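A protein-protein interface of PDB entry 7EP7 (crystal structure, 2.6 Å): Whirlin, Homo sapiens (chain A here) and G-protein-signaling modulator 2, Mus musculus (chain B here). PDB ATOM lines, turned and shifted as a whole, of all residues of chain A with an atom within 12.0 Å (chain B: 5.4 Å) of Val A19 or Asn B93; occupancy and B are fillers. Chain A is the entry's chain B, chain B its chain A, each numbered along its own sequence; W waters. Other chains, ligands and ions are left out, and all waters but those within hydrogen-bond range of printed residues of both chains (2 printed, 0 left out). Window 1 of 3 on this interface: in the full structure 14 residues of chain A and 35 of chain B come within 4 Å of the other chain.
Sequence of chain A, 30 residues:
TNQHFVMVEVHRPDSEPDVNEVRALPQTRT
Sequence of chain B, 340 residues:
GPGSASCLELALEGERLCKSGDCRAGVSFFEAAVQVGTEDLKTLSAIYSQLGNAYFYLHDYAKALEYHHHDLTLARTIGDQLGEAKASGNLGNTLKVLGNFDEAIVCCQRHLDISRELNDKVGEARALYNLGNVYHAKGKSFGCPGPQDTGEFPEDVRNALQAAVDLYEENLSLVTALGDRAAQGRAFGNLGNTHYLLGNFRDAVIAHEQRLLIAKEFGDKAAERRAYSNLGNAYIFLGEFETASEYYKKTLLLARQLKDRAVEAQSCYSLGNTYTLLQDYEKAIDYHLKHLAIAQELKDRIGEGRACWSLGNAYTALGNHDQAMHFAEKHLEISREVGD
Water W2 lies within hydrogen-bond range of ND2 of Asn B130 (2.7 Å), O of Val A19 (3.2 Å), OD1 of Asn B93 (3.3 Å) and N of Glu A21 (3.3 Å).
Water W1 lies within hydrogen-bond range of the side-chain amide oxygen of Asn B130 (2.9 Å), the side-chain amide nitrogen of Asn B133 (3.0 Å) and the backbone NH of Val A19 (3.1 Å).
Along chain B the printed residues that touch a printed residue of chain A span positions 56 to 186.
Of the 9 printed residues of chain A, 6 touch a printed residue of chain B.
OH of Tyr B129 touches CB of Glu A16, at 3.5 Å.
Glu A16 touches Arg B186 (CG to O, 3.4 Å).
CG of Pro A17 touches CD of Arg B186, 3.9 Å away.
Phe B56 touches Asp A18.
Asp A18 touches Asn B133 (OD1 to ND2, 3.9 Å).
OD1 of Asn B93 touches O of Val A19 (3.6 Å).
Val A19 touches Tyr B129.
Asn B130 touches Val A19 (OD1 to O, 3.5 Å).
Val A19 touches Arg B186.
Asn A20 touches Asn B93.
O of Gly B89 sits close to OD1 of Asn B93, at 3.4 Å.
OG1 of Thr B94 lies within hydrogen-bond range of O of Asn B90, at 2.8 Å.
The side-chain amide oxygen of Asn B130 lies close to the side-chain amide oxygen of Asn B93.
The backbone carbonyl oxygen (O) of Arg B126 lies close to the side-chain amide nitrogen (ND2) of Asn B130, at 3.4 Å.
ND2 of Asn A20 sits at hydrogen-bond distance from OD1 of Asn B90, 3.0 Å away.
OD1 of Asn B90 sits at hydrogen-bond distance from N of Glu A21.
The side-chain amino group (NZ) of Lys B96 lies within salt-bridge range of the side-chain carboxylate (OD1) of Asp A18, 2.7 Å away.
NE of Arg B126 lies within salt-bridge range of OE2 of Glu A21 (2.5 Å).
O of Pro A17 sits at hydrogen-bond distance from OH of Tyr B129 (2.8 Å).
Of chain A, only Val A19 (3.6 Å) and Asn A20 (3.8 Å) come within 4 Å of Asn B93.
No residue of chain A comes within 4 Å of Gly B89.
Asn B90 touches just these residues of chain A: Asn A20 (3.0 Å) and Glu A21 (2.9 Å).
No residue of chain A comes within 4 Å of Gly B92.
No residue of chain A comes within 4 Å of Thr B94.
No residue of chain A comes within 4 Å of Leu B95.
Lys B96 touches one residue of chain A.
No residue of chain A comes within 4 Å of Val B97.
Of chain A, only Val A19 (3.5 Å) comes within 4 Å of Asn B130.
Asn B133 touches just one residue of chain A: Asp A18 (3.9 Å).
Of the printed residues of chain A, Phe B56 touches Asp A18 and Asn A20.
Printed residues of chain B within 4 Å of Asp A18: Phe B56, Lys B96 and Asn B133.
Arg A23 touches none of the printed residues of chain B.
The nearest residue of chain B that does not touch Val A19 is Arg B126 (4.6 Å).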
ATOM      1  N   SER A  15     -10.561  28.108 -43.232  1.00  0.00           N
ATOM      2  CA  SER A  15     -10.446  26.884 -42.458  1.00  0.00           C
ATOM      3  C   SER A  15     -11.835  26.362 -42.105  1.00  0.00           C
ATOM      4  O   SER A  15     -12.859  26.840 -42.591  1.00  0.00           O
ATOM      5  CB  SER A  15      -9.602  27.111 -41.198  1.00  0.00           C
ATOM      6  OG  SER A  15     -10.253  27.977 -40.273  1.00  0.00           O
ATOM      7  N   GLU A  16     -11.866  25.390 -41.258  1.00  0.00           N
ATOM      8  CA  GLU A  16     -12.997  24.720 -40.689  1.00  0.00           C
ATOM      9  C   GLU A  16     -13.149  25.115 -39.228  1.00  0.00           C
ATOM     10  O   GLU A  16     -12.156  25.387 -38.539  1.00  0.00           O
ATOM     11  CB  GLU A  16     -12.823  23.200 -40.805  1.00  0.00           C
ATOM     12  CG  GLU A  16     -12.716  22.759 -42.252  1.00  0.00           C
ATOM     13  CD  GLU A  16     -13.997  23.032 -43.042  1.00  0.00           C
ATOM     14  OE1 GLU A  16     -15.111  22.726 -42.536  1.00  0.00           O
ATOM     15  OE2 GLU A  16     -13.876  23.615 -44.148  1.00  0.00           O
ATOM     16  N   PRO A  17     -14.380  25.141 -38.727  1.00  0.00           N
ATOM     17  CA  PRO A  17     -14.603  25.559 -37.343  1.00  0.00           C
ATOM     18  C   PRO A  17     -14.014  24.589 -36.329  1.00  0.00           C
ATOM     19  O   PRO A  17     -14.018  23.365 -36.501  1.00  0.00           O
ATOM     20  CB  PRO A  17     -16.132  25.595 -37.220  1.00  0.00           C
ATOM     21  CG  PRO A  17     -16.597  24.615 -38.277  1.00  0.00           C
ATOM     22  CD  PRO A  17     -15.638  24.816 -39.415  1.00  0.00           C
ATOM     23  N   ASP A  18     -13.719  25.184 -35.193  1.00  0.00           N
ATOM     24  CA  ASP A  18     -13.285  24.367 -34.055  1.00  0.00           C
ATOM     25  C   ASP A  18     -14.558  23.728 -33.547  1.00  0.00           C
ATOM     26  O   ASP A  18     -15.636  24.234 -33.841  1.00  0.00           O
ATOM     27  CB  ASP A  18     -12.644  25.242 -32.982  1.00  0.00           C
ATOM     28  CG  ASP A  18     -11.537  26.142 -33.501  1.00  0.00           C
ATOM     29  OD1 ASP A  18     -10.574  25.606 -34.056  1.00  0.00           O
ATOM     30  OD2 ASP A  18     -11.649  27.368 -33.342  1.00  0.00           O
ATOM     31  N   VAL A  19     -14.422  22.674 -32.788  1.00  0.00           N
ATOM     32  CA  VAL A  19     -15.567  21.897 -32.305  1.00  0.00           C
ATOM     33  C   VAL A  19     -15.323  21.547 -30.847  1.00  0.00           C
ATOM     34  O   VAL A  19     -14.552  20.622 -30.544  1.00  0.00           O
ATOM     35  CB  VAL A  19     -15.831  20.611 -33.102  1.00  0.00           C
ATOM     36  CG1 VAL A  19     -17.009  19.817 -32.425  1.00  0.00           C
ATOM     37  CG2 VAL A  19     -16.076  20.911 -34.594  1.00  0.00           C
ATOM     38  N   ASN A  20     -16.028  22.233 -29.953  1.00  0.00           N
ATOM     39  CA  ASN A  20     -15.861  22.044 -28.524  1.00  0.00           C
ATOM     40  C   ASN A  20     -16.800  20.945 -28.025  1.00  0.00           C
ATOM     41  O   ASN A  20     -17.774  20.574 -28.677  1.00  0.00           O
ATOM     42  CB  ASN A  20     -16.105  23.360 -27.773  1.00  0.00           C
ATOM     43  CG  ASN A  20     -14.948  24.384 -27.941  1.00  0.00           C
ATOM     44  OD1 ASN A  20     -14.931  25.200 -28.879  1.00  0.00           O
ATOM     45  ND2 ASN A  20     -13.986  24.339 -27.016  1.00  0.00           N
ATOM     46  N   GLU A  21     -16.463  20.406 -26.863  1.00  0.00           N
ATOM     47  CA  GLU A  21     -17.248  19.391 -26.185  1.00  0.00           C
ATOM     48  C   GLU A  21     -18.374  20.065 -25.424  1.00  0.00           C
ATOM     49  O   GLU A  21     -18.152  21.055 -24.712  1.00  0.00           O
ATOM     50  CB  GLU A  21     -16.381  18.605 -25.203  1.00  0.00           C
ATOM     51  CG  GLU A  21     -15.419  17.679 -25.863  1.00  0.00           C
ATOM     52  CD  GLU A  21     -16.087  16.362 -26.137  1.00  0.00           C
ATOM     53  OE1 GLU A  21     -17.178  16.139 -25.565  1.00  0.00           O
ATOM     54  OE2 GLU A  21     -15.538  15.564 -26.929  1.00  0.00           O
ATOM     55  N   VAL A  22     -19.567  19.517 -25.554  1.00  0.00           N
ATOM     56  CA  VAL A  22     -20.719  20.039 -24.846  1.00  0.00           C
ATOM     57  C   VAL A  22     -21.025  19.069 -23.712  1.00  0.00           C
ATOM     58  O   VAL A  22     -20.871  17.846 -23.849  1.00  0.00           O
ATOM     59  CB  VAL A  22     -21.907  20.273 -25.800  1.00  0.00           C
ATOM     60  CG1 VAL A  22     -23.122  20.757 -25.034  1.00  0.00           C
ATOM     61  CG2 VAL A  22     -21.490  21.334 -26.838  1.00  0.00           C
ATOM     62  N   ARG A  23     -21.375  19.628 -22.555  1.00  0.00           N
ATOM     63  CA  ARG A  23     -21.537  18.866 -21.323  1.00  0.00           C
ATOM     64  C   ARG A  23     -22.929  19.260 -20.802  1.00  0.00           C
ATOM     65  O   ARG A  23     -23.063  20.126 -19.928  1.00  0.00           O
ATOM     66  CB  ARG A  23     -20.359  19.191 -20.370  1.00  0.00           C
ATOM     67  CG  ARG A  23     -20.245  18.416 -19.069  1.00  0.00           C
ATOM     68  CD  ARG A  23     -18.854  18.644 -18.468  1.00  0.00           C
ATOM     69  NE  ARG A  23     -18.852  18.465 -17.016  1.00  0.00           N
ATOM     70  CZ  ARG A  23     -18.934  17.287 -16.400  1.00  0.00           C
ATOM     71  NH1 ARG A  23     -19.012  16.155 -17.117  1.00  0.00           N
ATOM     72  NH2 ARG A  23     -18.948  17.244 -15.063  1.00  0.00           N
ATOM     73  N   PHE B  56     -16.467  31.222 -25.706  1.00  0.00           N
ATOM     74  CA  PHE B  56     -15.764  30.830 -26.926  1.00  0.00           C
ATOM     75  C   PHE B  56     -16.460  31.359 -28.181  1.00  0.00           C
ATOM     76  O   PHE B  56     -15.865  32.116 -28.961  1.00  0.00           O
ATOM     77  CB  PHE B  56     -15.625  29.308 -26.999  1.00  0.00           C
ATOM     78  CG  PHE B  56     -14.593  28.853 -27.991  1.00  0.00           C
ATOM     79  CD1 PHE B  56     -13.244  28.723 -27.611  1.00  0.00           C
ATOM     80  CD2 PHE B  56     -14.953  28.548 -29.303  1.00  0.00           C
ATOM     81  CE1 PHE B  56     -12.263  28.312 -28.539  1.00  0.00           C
ATOM     82  CE2 PHE B  56     -13.974  28.119 -30.245  1.00  0.00           C
ATOM     83  CZ  PHE B  56     -12.622  28.007 -29.856  1.00  0.00           C
ATOM     84  N   SER B  88     -10.523  19.348 -20.523  1.00  0.00           N
ATOM     85  CA  SER B  88      -9.198  19.366 -21.163  1.00  0.00           C
ATOM     86  C   SER B  88      -9.280  19.700 -22.650  1.00  0.00           C
ATOM     87  O   SER B  88      -8.473  20.492 -23.166  1.00  0.00           O
ATOM     88  CB  SER B  88      -8.510  18.004 -20.998  1.00  0.00           C
ATOM     89  OG  SER B  88      -7.992  17.832 -19.711  1.00  0.00           O
ATOM     90  N   GLY B  89     -10.207  19.066 -23.373  1.00  0.00           N
ATOM     91  CA  GLY B  89     -10.386  19.424 -24.775  1.00  0.00           C
ATOM     92  C   GLY B  89     -10.748  20.889 -24.966  1.00  0.00           C
ATOM     93  O   GLY B  89     -10.253  21.549 -25.891  1.00  0.00           O
ATOM     94  N   ASN B  90     -11.618  21.423 -24.090  1.00  0.00           N
ATOM     95  CA  ASN B  90     -12.110  22.778 -24.282  1.00  0.00           C
ATOM     96  C   ASN B  90     -11.037  23.780 -23.904  1.00  0.00           C
ATOM     97  O   ASN B  90     -10.860  24.805 -24.584  1.00  0.00           O
ATOM     98  CB  ASN B  90     -13.390  22.980 -23.465  1.00  0.00           C
ATOM     99  CG  ASN B  90     -14.614  22.239 -24.069  1.00  0.00           C
ATOM    100  OD1 ASN B  90     -14.697  22.014 -25.286  1.00  0.00           O
ATOM    101  ND2 ASN B  90     -15.554  21.858 -23.213  1.00  0.00           N
ATOM    102  N   LEU B  91     -10.312  23.497 -22.815  1.00  0.00           N
ATOM    103  CA  LEU B  91      -9.109  24.247 -22.488  1.00  0.00           C
ATOM    104  C   LEU B  91      -8.156  24.248 -23.667  1.00  0.00           C
ATOM    105  O   LEU B  91      -7.692  25.307 -24.116  1.00  0.00           O
ATOM    106  CB  LEU B  91      -8.434  23.623 -21.270  1.00  0.00           C
ATOM    107  CG  LEU B  91      -8.891  24.242 -19.969  1.00  0.00           C
ATOM    108  CD1 LEU B  91      -8.310  23.488 -18.782  1.00  0.00           C
ATOM    109  CD2 LEU B  91      -8.462  25.707 -20.006  1.00  0.00           C
ATOM    110  N   GLY B  92      -7.864  23.044 -24.179  1.00  0.00           N
ATOM    111  CA  GLY B  92      -7.025  22.912 -25.356  1.00  0.00           C
ATOM    112  C   GLY B  92      -7.435  23.829 -26.483  1.00  0.00           C
ATOM    113  O   GLY B  92      -6.623  24.624 -26.970  1.00  0.00           O
ATOM    114  N   ASN B  93      -8.711  23.766 -26.889  1.00  0.00           N
ATOM    115  CA  ASN B  93      -9.126  24.556 -28.054  1.00  0.00           C
ATOM    116  C   ASN B  93      -9.070  26.039 -27.748  1.00  0.00           C
ATOM    117  O   ASN B  93      -8.671  26.839 -28.600  1.00  0.00           O
ATOM    118  CB  ASN B  93     -10.523  24.154 -28.546  1.00  0.00           C
ATOM    119  CG  ASN B  93     -10.610  22.664 -28.972  1.00  0.00           C
ATOM    120  OD1 ASN B  93     -11.688  22.072 -28.947  1.00  0.00           O
ATOM    121  ND2 ASN B  93      -9.472  22.062 -29.332  1.00  0.00           N
ATOM    122  N   THR B  94      -9.401  26.422 -26.517  1.00  0.00           N
ATOM    123  CA  THR B  94      -9.274  27.821 -26.126  1.00  0.00           C
ATOM    124  C   THR B  94      -7.812  28.268 -26.159  1.00  0.00           C
ATOM    125  O   THR B  94      -7.484  29.307 -26.748  1.00  0.00           O
ATOM    126  CB  THR B  94      -9.888  28.018 -24.739  1.00  0.00           C
ATOM    127  OG1 THR B  94     -11.233  27.526 -24.757  1.00  0.00           O
ATOM    128  CG2 THR B  94      -9.931  29.455 -24.395  1.00  0.00           C
ATOM    129  N   LEU B  95      -6.913  27.485 -25.539  1.00  0.00           N
ATOM    130  CA  LEU B  95      -5.487  27.840 -25.541  1.00  0.00           C
ATOM    131  C   LEU B  95      -4.945  27.935 -26.955  1.00  0.00           C
ATOM    132  O   LEU B  95      -4.137  28.820 -27.257  1.00  0.00           O
ATOM    133  CB  LEU B  95      -4.654  26.831 -24.742  1.00  0.00           C
ATOM    134  CG  LEU B  95      -4.958  26.765 -23.246  1.00  0.00           C
ATOM    135  CD1 LEU B  95      -4.648  25.394 -22.598  1.00  0.00           C
ATOM    136  CD2 LEU B  95      -4.248  27.892 -22.532  1.00  0.00           C
ATOM    137  N   LYS B  96      -5.386  27.039 -27.836  1.00  0.00           N
ATOM    138  CA  LYS B  96      -4.954  27.095 -29.229  1.00  0.00           C
ATOM    139  C   LYS B  96      -5.240  28.459 -29.837  1.00  0.00           C
ATOM    140  O   LYS B  96      -4.398  29.028 -30.544  1.00  0.00           O
ATOM    141  CB  LYS B  96      -5.650  25.977 -30.012  1.00  0.00           C
ATOM    142  CG  LYS B  96      -5.174  25.809 -31.424  1.00  0.00           C
ATOM    143  CD  LYS B  96      -6.052  26.497 -32.394  1.00  0.00           C
ATOM    144  CE  LYS B  96      -7.289  25.712 -32.698  1.00  0.00           C
ATOM    145  NZ  LYS B  96      -8.026  26.429 -33.816  1.00  0.00           N
ATOM    146  N   VAL B  97      -6.419  29.015 -29.555  1.00  0.00           N
ATOM    147  CA  VAL B  97      -6.802  30.288 -30.164  1.00  0.00           C
ATOM    148  C   VAL B  97      -5.964  31.425 -29.598  1.00  0.00           C
ATOM    149  O   VAL B  97      -5.555  32.340 -30.322  1.00  0.00           O
ATOM    150  CB  VAL B  97      -8.313  30.516 -29.961  1.00  0.00           C
ATOM    151  CG1 VAL B  97      -8.700  31.990 -30.161  1.00  0.00           C
ATOM    152  CG2 VAL B  97      -9.107  29.600 -30.901  1.00  0.00           C
ATOM    153  N   CYS B 108      -5.185  18.806 -25.128  1.00  0.00           N
ATOM    154  CA  CYS B 108      -5.872  17.944 -26.077  1.00  0.00           C
ATOM    155  C   CYS B 108      -5.405  16.498 -25.914  1.00  0.00           C
ATOM    156  O   CYS B 108      -6.218  15.562 -25.952  1.00  0.00           O
ATOM    157  CB  CYS B 108      -5.667  18.466 -27.495  1.00  0.00           C
ATOM    158  SG  CYS B 108      -6.425  20.154 -27.723  1.00  0.00           S
ATOM    159  N   ARG B 126     -13.010  13.320 -31.586  1.00  0.00           N
ATOM    160  CA  ARG B 126     -13.035  14.758 -31.324  1.00  0.00           C
ATOM    161  C   ARG B 126     -11.691  15.236 -30.787  1.00  0.00           C
ATOM    162  O   ARG B 126     -11.125  16.230 -31.271  1.00  0.00           O
ATOM    163  CB  ARG B 126     -14.175  15.087 -30.357  1.00  0.00           C
ATOM    164  CG  ARG B 126     -15.550  15.050 -31.050  1.00  0.00           C
ATOM    165  CD  ARG B 126     -16.669  15.724 -30.291  1.00  0.00           C
ATOM    166  NE  ARG B 126     -16.842  15.121 -28.982  1.00  0.00           N
ATOM    167  CZ  ARG B 126     -17.985  14.609 -28.523  1.00  0.00           C
ATOM    168  NH1 ARG B 126     -19.077  14.608 -29.291  1.00  0.00           N
ATOM    169  NH2 ARG B 126     -18.022  14.061 -27.304  1.00  0.00           N
ATOM    170  N   TYR B 129      -9.256  15.460 -33.773  1.00  0.00           N
ATOM    171  CA  TYR B 129      -9.475  16.673 -34.562  1.00  0.00           C
ATOM    172  C   TYR B 129      -8.943  17.923 -33.849  1.00  0.00           C
ATOM    173  O   TYR B 129      -8.339  18.788 -34.493  1.00  0.00           O
ATOM    174  CB  TYR B 129     -10.965  16.816 -34.864  1.00  0.00           C
ATOM    175  CG  TYR B 129     -11.355  18.058 -35.627  1.00  0.00           C
ATOM    176  CD1 TYR B 129     -11.164  18.127 -37.006  1.00  0.00           C
ATOM    177  CD2 TYR B 129     -11.947  19.159 -34.981  1.00  0.00           C
ATOM    178  CE1 TYR B 129     -11.522  19.261 -37.736  1.00  0.00           C
ATOM    179  CE2 TYR B 129     -12.333  20.286 -35.705  1.00  0.00           C
ATOM    180  CZ  TYR B 129     -12.110  20.329 -37.084  1.00  0.00           C
ATOM    181  OH  TYR B 129     -12.463  21.430 -37.838  1.00  0.00           O
ATOM    182  N   ASN B 130      -9.168  18.039 -32.523  1.00  0.00           N
ATOM    183  CA  ASN B 130      -8.603  19.143 -31.740  1.00  0.00           C
ATOM    184  C   ASN B 130      -7.074  19.159 -31.791  1.00  0.00           C
ATOM    185  O   ASN B 130      -6.453  20.198 -32.059  1.00  0.00           O
ATOM    186  CB  ASN B 130      -9.048  19.032 -30.291  1.00  0.00           C
ATOM    187  CG  ASN B 130     -10.511  19.281 -30.114  1.00  0.00           C
ATOM    188  OD1 ASN B 130     -11.140  19.916 -30.964  1.00  0.00           O
ATOM    189  ND2 ASN B 130     -11.077  18.782 -28.991  1.00  0.00           N
ATOM    190  N   ASN B 133      -5.865  20.399 -35.022  1.00  0.00           N
ATOM    191  CA  ASN B 133      -6.022  21.839 -35.168  1.00  0.00           C
ATOM    192  C   ASN B 133      -4.903  22.590 -34.461  1.00  0.00           C
ATOM    193  O   ASN B 133      -4.437  23.607 -34.971  1.00  0.00           O
ATOM    194  CB  ASN B 133      -7.392  22.264 -34.634  1.00  0.00           C
ATOM    195  CG  ASN B 133      -8.511  21.896 -35.582  1.00  0.00           C
ATOM    196  OD1 ASN B 133      -8.266  21.489 -36.727  1.00  0.00           O
ATOM    197  ND2 ASN B 133      -9.739  21.956 -35.093  1.00  0.00           N
ATOM    198  N   VAL B 134      -4.454  22.107 -33.288  1.00  0.00           N
ATOM    199  CA  VAL B 134      -3.380  22.815 -32.583  1.00  0.00           C
ATOM    200  C   VAL B 134      -2.114  22.800 -33.417  1.00  0.00           C
ATOM    201  O   VAL B 134      -1.565  23.852 -33.760  1.00  0.00           O
ATOM    202  CB  VAL B 134      -3.112  22.221 -31.193  1.00  0.00           C
ATOM    203  CG1 VAL B 134      -1.934  22.933 -30.612  1.00  0.00           C
ATOM    204  CG2 VAL B 134      -4.293  22.393 -30.275  1.00  0.00           C
ATOM    205  N   ARG B 186     -15.210  18.549 -42.088  1.00  0.00           N
ATOM    206  CA  ARG B 186     -14.291  19.377 -41.333  1.00  0.00           C
ATOM    207  C   ARG B 186     -12.874  18.820 -41.389  1.00  0.00           C
ATOM    208  O   ARG B 186     -11.910  19.572 -41.594  1.00  0.00           O
ATOM    209  CB  ARG B 186     -14.803  19.487 -39.901  1.00  0.00           C
ATOM    210  CG  ARG B 186     -16.104  20.250 -39.876  1.00  0.00           C
ATOM    211  CD  ARG B 186     -16.541  20.699 -38.502  1.00  0.00           C
ATOM    212  NE  ARG B 186     -16.829  19.605 -37.598  1.00  0.00           N
ATOM    213  CZ  ARG B 186     -18.019  19.021 -37.508  1.00  0.00           C
ATOM    214  NH1 ARG B 186     -19.015  19.414 -38.302  1.00  0.00           N
ATOM    215  NH2 ARG B 186     -18.200  18.044 -36.628  1.00  0.00           N
HETATM  216  O   HOH W   1     -11.369  22.272 -32.570  1.00  0.00           O
HETATM  217  O   HOH W   2     -13.400  19.573 -27.758  1.00  0.00           O
